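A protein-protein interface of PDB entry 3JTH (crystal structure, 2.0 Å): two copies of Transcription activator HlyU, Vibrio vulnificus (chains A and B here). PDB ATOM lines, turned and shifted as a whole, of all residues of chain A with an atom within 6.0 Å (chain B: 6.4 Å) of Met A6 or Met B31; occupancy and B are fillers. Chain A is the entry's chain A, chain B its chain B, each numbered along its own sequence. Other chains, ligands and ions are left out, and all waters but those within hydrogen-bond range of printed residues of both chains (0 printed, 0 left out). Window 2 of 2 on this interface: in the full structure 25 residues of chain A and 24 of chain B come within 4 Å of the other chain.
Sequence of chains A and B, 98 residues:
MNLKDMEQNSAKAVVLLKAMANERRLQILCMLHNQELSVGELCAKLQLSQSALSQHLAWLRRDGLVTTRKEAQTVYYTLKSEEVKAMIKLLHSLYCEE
The side-chain amide oxygen of Gln B27 lies within hydrogen-bond range of the side-chain hydroxyl of Ser A10 (3.0 Å).
The backbone carbonyl oxygen (O) of Met B31 is in hydrogen-bond range of the side-chain amide nitrogen (NE2) of Gln B35, at 2.5 Å. O of Met A6 lies close to OG of Ser A10 (3.1 Å). The backbone carbonyl oxygen (O) of Leu B26 is in hydrogen-bond range of the side-chain sulfur (SG) of Cys B30. The side-chain amino group (NZ) of Lys B45 is in hydrogen-bond range of the side-chain sulfur (SD) of Met B31 (3.4 Å). The side-chain hydroxyl of Ser A10 is in hydrogen-bond range of the backbone carbonyl oxygen of Glu A7, at 2.9 Å.
Among the printed residues, pairs that only touch across the chains: Met A6 with Gln B27 (3.7 Å), Met A6 with Met B31 (3.3 Å), Met A6 with Leu B46 (3.5 Å) and Ser A10 with Leu B26 (3.9 Å).
Of chain B, only Gln B27 (3.7 Å), Met B31 (3.3 Å) and Leu B46 (3.5 Å) come within 4 Å of Met A6. Of the printed residues of chain B, Ser A10 touches Leu B26 (3.9 Å) and Gln B27 (3.0 Å). Ala A11 touches none of the printed residues of chain B. Of the printed residues of chain A, Leu B26 touches Ser A10 (3.9 Å). Printed residues of chain A within 4 Å of Gln B27: Met A6 (3.7 Å) and Ser A10 (3.0 Å). Of chain A, only Met A6 (3.3 Å) comes within 4 Å of Met B31. Leu B42 touches none of the printed residues of chain A. The nearest residue of chain B that does not touch Met A6 is Lys B45 (4.4 Å). The nearest printed residue of chain A that does not touch Met B31 is Asn A2 (7.2 Å). The nearest printed residue of chain B that does not touch Ser A10 is Cys B30 (6.3 Å).
Hydrophobic or aromatic side chains of chain A within 4 Å of the printed part of chain B: Met A6. Along chain A the printed residues that touch a printed residue of chain B span positions 6 to 10. Among the printed residues, no Asp or Glu carboxylate lies within 4 Å of a Lys or Arg side-chain nitrogen of the other chain.
No position is printed for both chains. Of the 5 pairs that touch across the chains among the printed residues, none has its exchanged pair printed and touching as well.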
ATOM      1  N   ASN A   2     -28.739 -27.243  21.033  1.00  0.00           N
ATOM      2  CA  ASN A   2     -27.354 -26.791  20.959  1.00  0.00           C
ATOM      3  C   ASN A   2     -26.368 -27.941  20.781  1.00  0.00           C
ATOM      4  O   ASN A   2     -25.185 -27.716  20.530  1.00  0.00           O
ATOM      5  CB  ASN A   2     -26.975 -26.001  22.212  1.00  0.00           C
ATOM      6  CG  ASN A   2     -25.782 -25.087  21.985  1.00  0.00           C
ATOM      7  OD1 ASN A   2     -24.771 -25.491  21.408  1.00  0.00           O
ATOM      8  ND2 ASN A   2     -25.894 -23.846  22.444  1.00  0.00           N
ATOM      9  N   LEU A   3     -26.841 -29.173  20.919  1.00  0.00           N
ATOM     10  CA  LEU A   3     -25.951 -30.311  20.748  1.00  0.00           C
ATOM     11  C   LEU A   3     -25.437 -30.344  19.315  1.00  0.00           C
ATOM     12  O   LEU A   3     -24.234 -30.445  19.074  1.00  0.00           O
ATOM     13  CB  LEU A   3     -26.676 -31.625  21.078  1.00  0.00           C
ATOM     14  CG  LEU A   3     -28.093 -31.875  20.545  1.00  0.00           C
ATOM     15  CD1 LEU A   3     -28.437 -33.354  20.662  1.00  0.00           C
ATOM     16  CD2 LEU A   3     -29.094 -31.036  21.330  1.00  0.00           C
ATOM     17  N   LYS A   4     -26.367 -30.228  18.372  1.00  0.00           N
ATOM     18  CA  LYS A   4     -26.058 -30.267  16.946  1.00  0.00           C
ATOM     19  C   LYS A   4     -25.229 -29.097  16.411  1.00  0.00           C
ATOM     20  O   LYS A   4     -24.467 -29.266  15.465  1.00  0.00           O
ATOM     21  CB  LYS A   4     -27.367 -30.395  16.159  1.00  0.00           C
ATOM     22  CG  LYS A   4     -28.179 -31.613  16.585  1.00  0.00           C
ATOM     23  CD  LYS A   4     -29.647 -31.475  16.238  1.00  0.00           C
ATOM     24  CE  LYS A   4     -30.507 -32.413  17.079  1.00  0.00           C
ATOM     25  NZ  LYS A   4     -30.258 -33.858  16.810  1.00  0.00           N
ATOM     26  N   ASP A   5     -25.366 -27.918  17.007  1.00  0.00           N
ATOM     27  CA  ASP A   5     -24.598 -26.763  16.547  1.00  0.00           C
ATOM     28  C   ASP A   5     -23.118 -27.007  16.825  1.00  0.00           C
ATOM     29  O   ASP A   5     -22.260 -26.748  15.982  1.00  0.00           O
ATOM     30  CB  ASP A   5     -25.058 -25.498  17.265  1.00  0.00           C
ATOM     31  CG  ASP A   5     -26.562 -25.436  17.415  1.00  0.00           C
ATOM     32  OD1 ASP A   5     -27.105 -26.267  18.172  1.00  0.00           O
ATOM     33  OD2 ASP A   5     -27.202 -24.572  16.777  1.00  0.00           O
ATOM     34  N   MET A   6     -22.834 -27.510  18.019  1.00  0.00           N
ATOM     35  CA  MET A   6     -21.472 -27.826  18.435  1.00  0.00           C
ATOM     36  C   MET A   6     -20.959 -29.019  17.625  1.00  0.00           C
ATOM     37  O   MET A   6     -19.780 -29.102  17.279  1.00  0.00           O
ATOM     38  CB  MET A   6     -21.468 -28.177  19.920  1.00  0.00           C
ATOM     39  CG  MET A   6     -20.154 -28.721  20.434  1.00  0.00           C
ATOM     40  SD  MET A   6     -20.464 -30.222  21.609  1.00  0.00           S
ATOM     41  CE  MET A   6     -21.688 -29.372  22.836  1.00  0.00           C
ATOM     42  N   GLU A   7     -21.873 -29.941  17.341  1.00  0.00           N
ATOM     43  CA  GLU A   7     -21.577 -31.147  16.580  1.00  0.00           C
ATOM     44  C   GLU A   7     -21.131 -30.837  15.151  1.00  0.00           C
ATOM     45  O   GLU A   7     -20.130 -31.371  14.668  1.00  0.00           O
ATOM     46  CB  GLU A   7     -22.823 -32.032  16.531  1.00  0.00           C
ATOM     47  CG  GLU A   7     -22.723 -33.222  15.593  1.00  0.00           C
ATOM     48  CD  GLU A   7     -24.067 -33.585  14.980  1.00  0.00           C
ATOM     49  OE1 GLU A   7     -24.537 -32.840  14.091  1.00  0.00           O
ATOM     50  OE2 GLU A   7     -24.657 -34.608  15.391  1.00  0.00           O
ATOM     51  N   GLN A   8     -21.887 -29.971  14.486  1.00  0.00           N
ATOM     52  CA  GLN A   8     -21.618 -29.598  13.106  1.00  0.00           C
ATOM     53  C   GLN A   8     -20.369 -28.744  12.946  1.00  0.00           C
ATOM     54  O   GLN A   8     -19.651 -28.861  11.949  1.00  0.00           O
ATOM     55  CB  GLN A   8     -22.834 -28.876  12.522  1.00  0.00           C
ATOM     56  CG  GLN A   8     -24.119 -29.700  12.595  1.00  0.00           C
ATOM     57  CD  GLN A   8     -25.310 -28.996  11.983  1.00  0.00           C
ATOM     58  OE1 GLN A   8     -25.350 -28.753  10.777  1.00  0.00           O
ATOM     59  NE2 GLN A   8     -26.291 -28.663  12.813  1.00  0.00           N
ATOM     60  N   ASN A   9     -20.100 -27.889  13.923  1.00  0.00           N
ATOM     61  CA  ASN A   9     -18.921 -27.043  13.837  1.00  0.00           C
ATOM     62  C   ASN A   9     -17.668 -27.797  14.253  1.00  0.00           C
ATOM     63  O   ASN A   9     -16.619 -27.619  13.646  1.00  0.00           O
ATOM     64  CB  ASN A   9     -19.107 -25.777  14.671  1.00  0.00           C
ATOM     65  CG  ASN A   9     -20.273 -24.938  14.180  1.00  0.00           C
ATOM     66  OD1 ASN A   9     -20.544 -24.885  12.979  1.00  0.00           O
ATOM     67  ND2 ASN A   9     -20.966 -24.278  15.104  1.00  0.00           N
ATOM     68  N   SER A  10     -17.769 -28.644  15.275  1.00  0.00           N
ATOM     69  CA  SER A  10     -16.614 -29.426  15.694  1.00  0.00           C
ATOM     70  C   SER A  10     -16.175 -30.228  14.467  1.00  0.00           C
ATOM     71  O   SER A  10     -14.982 -30.441  14.240  1.00  0.00           O
ATOM     72  CB  SER A  10     -16.983 -30.379  16.841  1.00  0.00           C
ATOM     73  OG  SER A  10     -17.848 -31.416  16.407  1.00  0.00           O
ATOM     74  N   ALA A  11     -17.149 -30.659  13.669  1.00  0.00           N
ATOM     75  CA  ALA A  11     -16.853 -31.414  12.460  1.00  0.00           C
ATOM     76  C   ALA A  11     -16.104 -30.542  11.444  1.00  0.00           C
ATOM     77  O   ALA A  11     -15.140 -30.992  10.834  1.00  0.00           O
ATOM     78  CB  ALA A  11     -18.149 -31.958  11.844  1.00  0.00           C
ATOM     79  N   LEU B  26     -12.122 -32.967  20.412  1.00  0.00           N
ATOM     80  CA  LEU B  26     -12.193 -31.515  20.304  1.00  0.00           C
ATOM     81  C   LEU B  26     -13.290 -30.971  21.201  1.00  0.00           C
ATOM     82  O   LEU B  26     -13.066 -30.009  21.922  1.00  0.00           O
ATOM     83  CB  LEU B  26     -12.435 -31.092  18.851  1.00  0.00           C
ATOM     84  CG  LEU B  26     -12.332 -29.585  18.577  1.00  0.00           C
ATOM     85  CD1 LEU B  26     -10.985 -29.046  19.060  1.00  0.00           C
ATOM     86  CD2 LEU B  26     -12.528 -29.334  17.087  1.00  0.00           C
ATOM     87  N   GLN B  27     -14.467 -31.592  21.175  1.00  0.00           N
ATOM     88  CA  GLN B  27     -15.575 -31.142  22.025  1.00  0.00           C
ATOM     89  C   GLN B  27     -15.146 -31.147  23.500  1.00  0.00           C
ATOM     90  O   GLN B  27     -15.417 -30.205  24.248  1.00  0.00           O
ATOM     91  CB  GLN B  27     -16.792 -32.044  21.802  1.00  0.00           C
ATOM     92  CG  GLN B  27     -17.395 -31.869  20.408  1.00  0.00           C
ATOM     93  CD  GLN B  27     -18.155 -33.090  19.909  1.00  0.00           C
ATOM     94  OE1 GLN B  27     -18.326 -33.264  18.703  1.00  0.00           O
ATOM     95  NE2 GLN B  27     -18.620 -33.933  20.828  1.00  0.00           N
ATOM     96  N   ILE B  28     -14.458 -32.210  23.904  1.00  0.00           N
ATOM     97  CA  ILE B  28     -13.960 -32.337  25.269  1.00  0.00           C
ATOM     98  C   ILE B  28     -13.046 -31.154  25.592  1.00  0.00           C
ATOM     99  O   ILE B  28     -13.238 -30.464  26.593  1.00  0.00           O
ATOM    100  CB  ILE B  28     -13.172 -33.647  25.437  1.00  0.00           C
ATOM    101  CG1 ILE B  28     -14.110 -34.832  25.238  1.00  0.00           C
ATOM    102  CG2 ILE B  28     -12.526 -33.697  26.808  1.00  0.00           C
ATOM    103  CD1 ILE B  28     -13.426 -36.186  25.346  1.00  0.00           C
ATOM    104  N   LEU B  29     -12.044 -30.944  24.743  1.00  0.00           N
ATOM    105  CA  LEU B  29     -11.101 -29.834  24.893  1.00  0.00           C
ATOM    106  C   LEU B  29     -11.854 -28.505  24.919  1.00  0.00           C
ATOM    107  O   LEU B  29     -11.516 -27.598  25.686  1.00  0.00           O
ATOM    108  CB  LEU B  29     -10.097 -29.829  23.733  1.00  0.00           C
ATOM    109  CG  LEU B  29      -9.106 -31.001  23.691  1.00  0.00           C
ATOM    110  CD1 LEU B  29      -8.389 -31.027  22.343  1.00  0.00           C
ATOM    111  CD2 LEU B  29      -8.115 -30.875  24.859  1.00  0.00           C
ATOM    112  N   CYS B  30     -12.878 -28.394  24.077  1.00  0.00           N
ATOM    113  CA  CYS B  30     -13.682 -27.180  24.017  1.00  0.00           C
ATOM    114  C   CYS B  30     -14.404 -26.946  25.332  1.00  0.00           C
ATOM    115  O   CYS B  30     -14.595 -25.799  25.741  1.00  0.00           O
ATOM    116  CB  CYS B  30     -14.692 -27.245  22.862  1.00  0.00           C
ATOM    117  SG  CYS B  30     -13.947 -27.002  21.225  1.00  0.00           S
ATOM    118  N   MET B  31     -14.800 -28.030  25.997  1.00  0.00           N
ATOM    119  CA  MET B  31     -15.492 -27.925  27.282  1.00  0.00           C
ATOM    120  C   MET B  31     -14.504 -27.618  28.410  1.00  0.00           C
ATOM    121  O   MET B  31     -14.792 -26.821  29.301  1.00  0.00           O
ATOM    122  CB  MET B  31     -16.241 -29.228  27.593  1.00  0.00           C
ATOM    123  CG  MET B  31     -17.437 -29.501  26.686  1.00  0.00           C
ATOM    124  SD  MET B  31     -18.872 -28.212  26.914  1.00  0.00           S
ATOM    125  CE  MET B  31     -20.196 -29.021  25.773  1.00  0.00           C
ATOM    126  N   LEU B  32     -13.332 -28.240  28.350  1.00  0.00           N
ATOM    127  CA  LEU B  32     -12.306 -28.053  29.364  1.00  0.00           C
ATOM    128  C   LEU B  32     -11.582 -26.714  29.309  1.00  0.00           C
ATOM    129  O   LEU B  32     -10.858 -26.369  30.247  1.00  0.00           O
ATOM    130  CB  LEU B  32     -11.277 -29.182  29.289  1.00  0.00           C
ATOM    131  CG  LEU B  32     -11.803 -30.587  29.602  1.00  0.00           C
ATOM    132  CD1 LEU B  32     -10.703 -31.608  29.404  1.00  0.00           C
ATOM    133  CD2 LEU B  32     -12.334 -30.632  31.037  1.00  0.00           C
ATOM    134  N   HIS B  33     -11.763 -25.952  28.235  1.00  0.00           N
ATOM    135  CA  HIS B  33     -11.087 -24.661  28.154  1.00  0.00           C
ATOM    136  C   HIS B  33     -11.601 -23.684  29.223  1.00  0.00           C
ATOM    137  O   HIS B  33     -12.754 -23.241  29.189  1.00  0.00           O
ATOM    138  CB  HIS B  33     -11.248 -24.039  26.765  1.00  0.00           C
ATOM    139  CG  HIS B  33     -10.423 -22.807  26.567  1.00  0.00           C
ATOM    140  ND1 HIS B  33     -10.635 -21.648  27.287  1.00  0.00           N
ATOM    141  CD2 HIS B  33      -9.354 -22.562  25.774  1.00  0.00           C
ATOM    142  CE1 HIS B  33      -9.733 -20.748  26.946  1.00  0.00           C
ATOM    143  NE2 HIS B  33      -8.941 -21.277  26.029  1.00  0.00           N
ATOM    144  N   ASN B  34     -10.731 -23.357  30.171  1.00  0.00           N
ATOM    145  CA  ASN B  34     -11.069 -22.441  31.254  1.00  0.00           C
ATOM    146  C   ASN B  34     -12.227 -22.917  32.136  1.00  0.00           C
ATOM    147  O   ASN B  34     -13.239 -22.225  32.275  1.00  0.00           O
ATOM    148  CB  ASN B  34     -11.389 -21.049  30.696  1.00  0.00           C
ATOM    149  CG  ASN B  34     -10.425 -19.981  31.198  1.00  0.00           C
ATOM    150  OD1 ASN B  34      -9.764 -19.306  30.405  1.00  0.00           O
ATOM    151  ND2 ASN B  34     -10.338 -19.826  32.516  1.00  0.00           N
ATOM    152  N   GLN B  35     -12.063 -24.101  32.725  1.00  0.00           N
ATOM    153  CA  GLN B  35     -13.048 -24.690  33.636  1.00  0.00           C
ATOM    154  C   GLN B  35     -12.863 -26.191  33.851  1.00  0.00           C
ATOM    155  O   GLN B  35     -13.387 -27.011  33.092  1.00  0.00           O
ATOM    156  CB  GLN B  35     -14.489 -24.417  33.177  1.00  0.00           C
ATOM    157  CG  GLN B  35     -14.839 -24.883  31.777  1.00  0.00           C
ATOM    158  CD  GLN B  35     -16.319 -25.182  31.641  1.00  0.00           C
ATOM    159  OE1 GLN B  35     -17.124 -24.769  32.477  1.00  0.00           O
ATOM    160  NE2 GLN B  35     -16.686 -25.897  30.585  1.00  0.00           N
ATOM    161  N   GLU B  36     -12.117 -26.534  34.901  1.00  0.00           N
ATOM    162  CA  GLU B  36     -11.846 -27.920  35.275  1.00  0.00           C
ATOM    163  C   GLU B  36     -13.170 -28.669  35.420  1.00  0.00           C
ATOM    164  O   GLU B  36     -14.094 -28.186  36.073  1.00  0.00           O
ATOM    165  CB  GLU B  36     -11.094 -27.952  36.607  1.00  0.00           C
ATOM    166  CG  GLU B  36     -10.395 -29.267  36.918  1.00  0.00           C
ATOM    167  CD  GLU B  36      -9.869 -29.320  38.343  1.00  0.00           C
ATOM    168  OE1 GLU B  36      -8.960 -30.133  38.627  1.00  0.00           O
ATOM    169  OE2 GLU B  36     -10.380 -28.554  39.185  1.00  0.00           O
ATOM    170  N   LEU B  37     -13.262 -29.853  34.825  1.00  0.00           N
ATOM    171  CA  LEU B  37     -14.498 -30.626  34.897  1.00  0.00           C
ATOM    172  C   LEU B  37     -14.297 -32.081  35.262  1.00  0.00           C
ATOM    173  O   LEU B  37     -13.248 -32.678  34.988  1.00  0.00           O
ATOM    174  CB  LEU B  37     -15.244 -30.541  33.559  1.00  0.00           C
ATOM    175  CG  LEU B  37     -15.746 -29.157  33.124  1.00  0.00           C
ATOM    176  CD1 LEU B  37     -16.095 -29.169  31.649  1.00  0.00           C
ATOM    177  CD2 LEU B  37     -16.956 -28.766  33.955  1.00  0.00           C
ATOM    178  N   LEU B  42     -18.718 -33.557  32.210  1.00  0.00           N
ATOM    179  CA  LEU B  42     -18.470 -33.565  30.776  1.00  0.00           C
ATOM    180  C   LEU B  42     -19.596 -34.339  30.106  1.00  0.00           C
ATOM    181  O   LEU B  42     -20.119 -33.915  29.067  1.00  0.00           O
ATOM    182  CB  LEU B  42     -17.121 -34.217  30.455  1.00  0.00           C
ATOM    183  CG  LEU B  42     -15.910 -33.292  30.582  1.00  0.00           C
ATOM    184  CD1 LEU B  42     -14.627 -34.102  30.544  1.00  0.00           C
ATOM    185  CD2 LEU B  42     -15.948 -32.254  29.451  1.00  0.00           C
ATOM    186  N   LYS B  45     -22.680 -32.154  30.096  1.00  0.00           N
ATOM    187  CA  LYS B  45     -22.559 -31.084  29.109  1.00  0.00           C
ATOM    188  C   LYS B  45     -22.519 -31.553  27.664  1.00  0.00           C
ATOM    189  O   LYS B  45     -22.978 -30.839  26.776  1.00  0.00           O
ATOM    190  CB  LYS B  45     -21.321 -30.220  29.391  1.00  0.00           C
ATOM    191  CG  LYS B  45     -21.301 -29.610  30.790  1.00  0.00           C
ATOM    192  CD  LYS B  45     -20.288 -28.488  30.914  1.00  0.00           C
ATOM    193  CE  LYS B  45     -20.881 -27.147  30.481  1.00  0.00           C
ATOM    194  NZ  LYS B  45     -21.316 -27.088  29.050  1.00  0.00           N
ATOM    195  N   LEU B  46     -21.977 -32.742  27.410  1.00  0.00           N
ATOM    196  CA  LEU B  46     -21.919 -33.256  26.041  1.00  0.00           C
ATOM    197  C   LEU B  46     -23.017 -34.267  25.766  1.00  0.00           C
ATOM    198  O   LEU B  46     -23.209 -34.689  24.625  1.00  0.00           O
ATOM    199  CB  LEU B  46     -20.559 -33.905  25.755  1.00  0.00           C
ATOM    200  CG  LEU B  46     -19.344 -32.987  25.646  1.00  0.00           C
ATOM    201  CD1 LEU B  46     -18.096 -33.825  25.490  1.00  0.00           C
ATOM    202  CD2 LEU B  46     -19.500 -32.065  24.461  1.00  0.00           C
ATOM    203  N   ILE B  88      -8.015 -23.347  20.745  1.00  0.00           N
ATOM    204  CA  ILE B  88      -9.432 -23.564  21.016  1.00  0.00           C
ATOM    205  C   ILE B  88     -10.175 -22.232  20.931  1.00  0.00           C
ATOM    206  O   ILE B  88     -11.230 -22.150  20.306  1.00  0.00           O
ATOM    207  CB  ILE B  88      -9.648 -24.192  22.404  1.00  0.00           C
ATOM    208  CG1 ILE B  88      -9.083 -25.612  22.406  1.00  0.00           C
ATOM    209  CG2 ILE B  88     -11.134 -24.195  22.762  1.00  0.00           C
ATOM    210  CD1 ILE B  88      -8.961 -26.208  23.775  1.00  0.00           C
